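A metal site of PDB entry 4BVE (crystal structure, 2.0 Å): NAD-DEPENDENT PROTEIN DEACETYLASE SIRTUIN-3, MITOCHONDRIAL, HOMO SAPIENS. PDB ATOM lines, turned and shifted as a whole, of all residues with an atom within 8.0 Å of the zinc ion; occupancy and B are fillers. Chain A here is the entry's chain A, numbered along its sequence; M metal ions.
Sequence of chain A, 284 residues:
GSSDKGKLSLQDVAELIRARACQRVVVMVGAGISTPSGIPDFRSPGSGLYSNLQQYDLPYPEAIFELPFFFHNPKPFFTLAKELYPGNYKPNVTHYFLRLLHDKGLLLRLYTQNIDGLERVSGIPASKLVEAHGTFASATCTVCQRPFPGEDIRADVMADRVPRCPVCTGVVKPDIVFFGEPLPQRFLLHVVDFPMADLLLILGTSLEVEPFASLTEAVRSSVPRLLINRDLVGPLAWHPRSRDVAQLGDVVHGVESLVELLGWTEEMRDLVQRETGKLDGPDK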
ATOM      1  N   THR A 140       0.027 -21.774 -10.829  1.00  0.00           N
ATOM      2  CA  THR A 140       0.006 -21.641 -12.324  1.00  0.00           C
ATOM      3  C   THR A 140      -1.067 -20.606 -12.677  1.00  0.00           C
ATOM      4  O   THR A 140      -2.163 -20.641 -12.106  1.00  0.00           O
ATOM      5  CB  THR A 140      -0.379 -23.000 -12.936  1.00  0.00           C
ATOM      6  OG1 THR A 140       0.579 -23.947 -12.511  1.00  0.00           O
ATOM      7  CG2 THR A 140      -0.405 -23.059 -14.439  1.00  0.00           C
ATOM      8  N   CYS A 141      -0.738 -19.648 -13.559  1.00  0.00           N
ATOM      9  CA  CYS A 141      -1.797 -18.752 -14.029  1.00  0.00           C
ATOM     10  C   CYS A 141      -2.910 -19.572 -14.698  1.00  0.00           C
ATOM     11  O   CYS A 141      -2.598 -20.363 -15.636  1.00  0.00           O
ATOM     12  CB  CYS A 141      -1.243 -17.775 -15.087  1.00  0.00           C
ATOM     13  SG  CYS A 141      -2.535 -16.659 -15.559  1.00  0.00           S
ATOM     14  N   THR A 142      -4.160 -19.355 -14.284  1.00  0.00           N
ATOM     15  CA  THR A 142      -5.270 -20.081 -14.864  1.00  0.00           C
ATOM     16  C   THR A 142      -5.566 -19.689 -16.333  1.00  0.00           C
ATOM     17  O   THR A 142      -6.222 -20.458 -17.076  1.00  0.00           O
ATOM     18  CB  THR A 142      -6.567 -19.836 -14.068  1.00  0.00           C
ATOM     19  OG1 THR A 142      -6.842 -18.420 -14.058  1.00  0.00           O
ATOM     20  CG2 THR A 142      -6.371 -20.366 -12.595  1.00  0.00           C
ATOM     21  N   VAL A 143      -4.988 -18.587 -16.770  1.00  0.00           N
ATOM     22  CA  VAL A 143      -5.225 -18.091 -18.121  1.00  0.00           C
ATOM     23  C   VAL A 143      -4.027 -18.471 -19.031  1.00  0.00           C
ATOM     24  O   VAL A 143      -4.161 -19.282 -19.993  1.00  0.00           O
ATOM     25  CB  VAL A 143      -5.477 -16.559 -18.160  1.00  0.00           C
ATOM     26  CG1 VAL A 143      -5.568 -16.073 -19.650  1.00  0.00           C
ATOM     27  CG2 VAL A 143      -6.764 -16.157 -17.408  1.00  0.00           C
ATOM     28  N   CYS A 144      -2.847 -17.919 -18.732  1.00  0.00           N
ATOM     29  CA  CYS A 144      -1.733 -18.114 -19.673  1.00  0.00           C
ATOM     30  C   CYS A 144      -0.889 -19.329 -19.330  1.00  0.00           C
ATOM     31  O   CYS A 144       0.038 -19.668 -20.086  1.00  0.00           O
ATOM     32  CB  CYS A 144      -0.836 -16.871 -19.759  1.00  0.00           C
ATOM     33  SG  CYS A 144       0.187 -16.568 -18.247  1.00  0.00           S
ATOM     34  N   GLN A 145      -1.207 -20.040 -18.226  1.00  0.00           N
ATOM     35  CA  GLN A 145      -0.426 -21.148 -17.730  1.00  0.00           C
ATOM     36  C   GLN A 145       1.029 -20.863 -17.318  1.00  0.00           C
ATOM     37  O   GLN A 145       1.755 -21.796 -17.149  1.00  0.00           O
ATOM     38  CB  GLN A 145      -0.409 -22.315 -18.750  1.00  0.00           C
ATOM     39  CG  GLN A 145      -1.761 -22.573 -19.443  1.00  0.00           C
ATOM     40  CD  GLN A 145      -2.762 -22.985 -18.420  1.00  0.00           C
ATOM     41  OE1 GLN A 145      -2.424 -23.727 -17.486  1.00  0.00           O
ATOM     42  NE2 GLN A 145      -3.986 -22.506 -18.555  1.00  0.00           N
ATOM     43  N   ARG A 146       1.475 -19.600 -17.131  1.00  0.00           N
ATOM     44  CA  ARG A 146       2.773 -19.358 -16.541  1.00  0.00           C
ATOM     45  C   ARG A 146       2.885 -19.980 -15.104  1.00  0.00           C
ATOM     46  O   ARG A 146       1.949 -19.843 -14.326  1.00  0.00           O
ATOM     47  CB  ARG A 146       3.054 -17.869 -16.493  1.00  0.00           C
ATOM     48  CG  ARG A 146       4.321 -17.511 -15.745  1.00  0.00           C
ATOM     49  CD  ARG A 146       4.774 -16.126 -16.214  1.00  0.00           C
ATOM     50  NE  ARG A 146       5.350 -15.260 -15.173  1.00  0.00           N
ATOM     51  CZ  ARG A 146       6.110 -14.200 -15.450  1.00  0.00           C
ATOM     52  NH1 ARG A 146       6.399 -13.914 -16.723  1.00  0.00           N
ATOM     53  NH2 ARG A 146       6.583 -13.417 -14.484  1.00  0.00           N
ATOM     54  N   PRO A 147       4.009 -20.677 -14.789  1.00  0.00           N
ATOM     55  CA  PRO A 147       4.256 -21.299 -13.465  1.00  0.00           C
ATOM     56  C   PRO A 147       4.873 -20.281 -12.507  1.00  0.00           C
ATOM     57  O   PRO A 147       5.526 -19.355 -12.984  1.00  0.00           O
ATOM     58  CB  PRO A 147       5.267 -22.435 -13.796  1.00  0.00           C
ATOM     59  CG  PRO A 147       6.059 -21.846 -14.990  1.00  0.00           C
ATOM     60  CD  PRO A 147       5.025 -21.078 -15.808  1.00  0.00           C
ATOM     61  N   PHE A 148       4.608 -20.387 -11.223  1.00  0.00           N
ATOM     62  CA  PHE A 148       5.191 -19.490 -10.236  1.00  0.00           C
ATOM     63  C   PHE A 148       5.594 -20.310  -9.027  1.00  0.00           C
ATOM     64  O   PHE A 148       4.851 -21.202  -8.605  1.00  0.00           O
ATOM     65  CB  PHE A 148       4.191 -18.382  -9.746  1.00  0.00           C
ATOM     66  CG  PHE A 148       3.688 -17.514 -10.873  1.00  0.00           C
ATOM     67  CD1 PHE A 148       4.437 -16.389 -11.301  1.00  0.00           C
ATOM     68  CD2 PHE A 148       2.558 -17.888 -11.611  1.00  0.00           C
ATOM     69  CE1 PHE A 148       4.028 -15.609 -12.412  1.00  0.00           C
ATOM     70  CE2 PHE A 148       2.127 -17.105 -12.694  1.00  0.00           C
ATOM     71  CZ  PHE A 148       2.863 -15.961 -13.080  1.00  0.00           C
ATOM     72  N   ARG A 164      -2.927 -12.492  -8.753  1.00  0.00           N
ATOM     73  CA  ARG A 164      -3.160 -12.231 -10.169  1.00  0.00           C
ATOM     74  C   ARG A 164      -1.824 -12.348 -10.952  1.00  0.00           C
ATOM     75  O   ARG A 164      -0.782 -12.074 -10.390  1.00  0.00           O
ATOM     76  CB  ARG A 164      -3.718 -10.805 -10.341  1.00  0.00           C
ATOM     77  CG  ARG A 164      -5.120 -10.637  -9.714  1.00  0.00           C
ATOM     78  CD  ARG A 164      -5.961 -11.282 -10.865  1.00  0.00           C
ATOM     79  NE  ARG A 164      -7.243 -11.393 -10.448  1.00  0.00           N
ATOM     80  CZ  ARG A 164      -8.290 -11.706 -11.179  1.00  0.00           C
ATOM     81  NH1 ARG A 164      -8.282 -11.925 -12.489  1.00  0.00           N
ATOM     82  NH2 ARG A 164      -9.358 -11.765 -10.477  1.00  0.00           N
ATOM     83  N   CYS A 165      -1.887 -12.648 -12.250  1.00  0.00           N
ATOM     84  CA  CYS A 165      -0.695 -12.934 -13.039  1.00  0.00           C
ATOM     85  C   CYS A 165      -0.076 -11.584 -13.483  1.00  0.00           C
ATOM     86  O   CYS A 165      -0.808 -10.732 -13.976  1.00  0.00           O
ATOM     87  CB  CYS A 165      -1.138 -13.741 -14.235  1.00  0.00           C
ATOM     88  SG  CYS A 165       0.162 -14.044 -15.424  1.00  0.00           S
ATOM     89  N   PRO A 166       1.234 -11.399 -13.318  1.00  0.00           N
ATOM     90  CA  PRO A 166       1.831 -10.124 -13.787  1.00  0.00           C
ATOM     91  C   PRO A 166       1.875  -9.975 -15.307  1.00  0.00           C
ATOM     92  O   PRO A 166       2.156  -8.862 -15.812  1.00  0.00           O
ATOM     93  CB  PRO A 166       3.269 -10.186 -13.243  1.00  0.00           C
ATOM     94  CG  PRO A 166       3.605 -11.679 -13.161  1.00  0.00           C
ATOM     95  CD  PRO A 166       2.279 -12.355 -12.801  1.00  0.00           C
ATOM     96  N   VAL A 167       1.615 -11.023 -16.038  1.00  0.00           N
ATOM     97  CA  VAL A 167       1.666 -10.957 -17.504  1.00  0.00           C
ATOM     98  C   VAL A 167       0.299 -10.727 -18.109  1.00  0.00           C
ATOM     99  O   VAL A 167       0.185  -9.976 -19.079  1.00  0.00           O
ATOM    100  CB  VAL A 167       2.241 -12.252 -18.159  1.00  0.00           C
ATOM    101  CG1 VAL A 167       2.258 -12.121 -19.687  1.00  0.00           C
ATOM    102  CG2 VAL A 167       3.650 -12.556 -17.648  1.00  0.00           C
ATOM    103  N   CYS A 168      -0.743 -11.421 -17.581  1.00  0.00           N
ATOM    104  CA  CYS A 168      -2.054 -11.416 -18.236  1.00  0.00           C
ATOM    105  C   CYS A 168      -3.172 -11.021 -17.298  1.00  0.00           C
ATOM    106  O   CYS A 168      -4.300 -10.810 -17.768  1.00  0.00           O
ATOM    107  CB  CYS A 168      -2.341 -12.755 -18.943  1.00  0.00           C
ATOM    108  SG  CYS A 168      -2.817 -14.035 -17.751  1.00  0.00           S
ATOM    109  N   THR A 169      -2.864 -10.794 -15.999  1.00  0.00           N
ATOM    110  CA  THR A 169      -3.855 -10.517 -14.916  1.00  0.00           C
ATOM    111  C   THR A 169      -4.791 -11.715 -14.604  1.00  0.00           C
ATOM    112  O   THR A 169      -5.662 -11.557 -13.765  1.00  0.00           O
ATOM    113  CB  THR A 169      -4.761  -9.238 -15.129  1.00  0.00           C
ATOM    114  OG1 THR A 169      -5.817  -9.509 -16.070  1.00  0.00           O
ATOM    115  CG2 THR A 169      -3.899  -8.010 -15.587  1.00  0.00           C
ATOM    116  N   GLY A 170      -4.590 -12.883 -15.200  1.00  0.00           N
ATOM    117  CA  GLY A 170      -5.399 -14.074 -14.844  1.00  0.00           C
ATOM    118  C   GLY A 170      -5.251 -14.419 -13.339  1.00  0.00           C
ATOM    119  O   GLY A 170      -4.221 -14.075 -12.684  1.00  0.00           O
ATOM    120  N   VAL A 171      -6.259 -15.132 -12.784  1.00  0.00           N
ATOM    121  CA  VAL A 171      -6.111 -15.666 -11.393  1.00  0.00           C
ATOM    122  C   VAL A 171      -4.990 -16.687 -11.327  1.00  0.00           C
ATOM    123  O   VAL A 171      -4.937 -17.600 -12.184  1.00  0.00           O
ATOM    124  CB  VAL A 171      -7.456 -16.306 -10.864  1.00  0.00           C
ATOM    125  CG1 VAL A 171      -7.263 -16.875  -9.449  1.00  0.00           C
ATOM    126  CG2 VAL A 171      -8.493 -15.226 -10.755  1.00  0.00           C
ATOM    127  N   VAL A 172      -4.057 -16.523 -10.373  1.00  0.00           N
ATOM    128  CA  VAL A 172      -2.937 -17.465 -10.217  1.00  0.00           C
ATOM    129  C   VAL A 172      -3.390 -18.522  -9.197  1.00  0.00           C
ATOM    130  O   VAL A 172      -3.697 -18.176  -8.025  1.00  0.00           O
ATOM    131  CB  VAL A 172      -1.634 -16.809  -9.812  1.00  0.00           C
ATOM    132  CG1 VAL A 172      -0.577 -17.904  -9.522  1.00  0.00           C
ATOM    133  CG2 VAL A 172      -1.117 -15.908 -10.987  1.00  0.00           C
HETATM  134 ZN    ZN M   1      -1.146 -15.186 -16.853  1.00  0.00          ZN
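O of Arg 146 sits at hydrogen-bond distance from N of Cys 141, 2.8 Å away.
N of Arg 146 sits close to SG of Cys 144.
N of Gly 170 lies close to SG of Cys 168.
The backbone NH of Val 143 sits close to the side-chain sulfur of Cys 141, 3.3 Å away.
SG of Cys 165 lies close to N of Val 167, at 3.4 Å.
The backbone carbonyl oxygen (O) of Gly 170 lies within hydrogen-bond range of the backbone NH (N) of Cys 165 (2.8 Å).
Of the 18 residues printed, 4 come within 4 Å of the zinc ion.
The nearest printed residue that does not touch the zinc ion is Gly 170 (4.5 Å).
The side-chain sulfur (SG) of Cys 168 is bound to the zinc ion.
SG of Cys 165 binds the zinc ion.
The zinc ion is bound by SG of Cys 144 (2.4 Å).
The side-chain sulfur (SG) of Cys 141 binds the zinc ion, at 2.4 Å.
The zinc ion has four donor atoms within binding distance.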
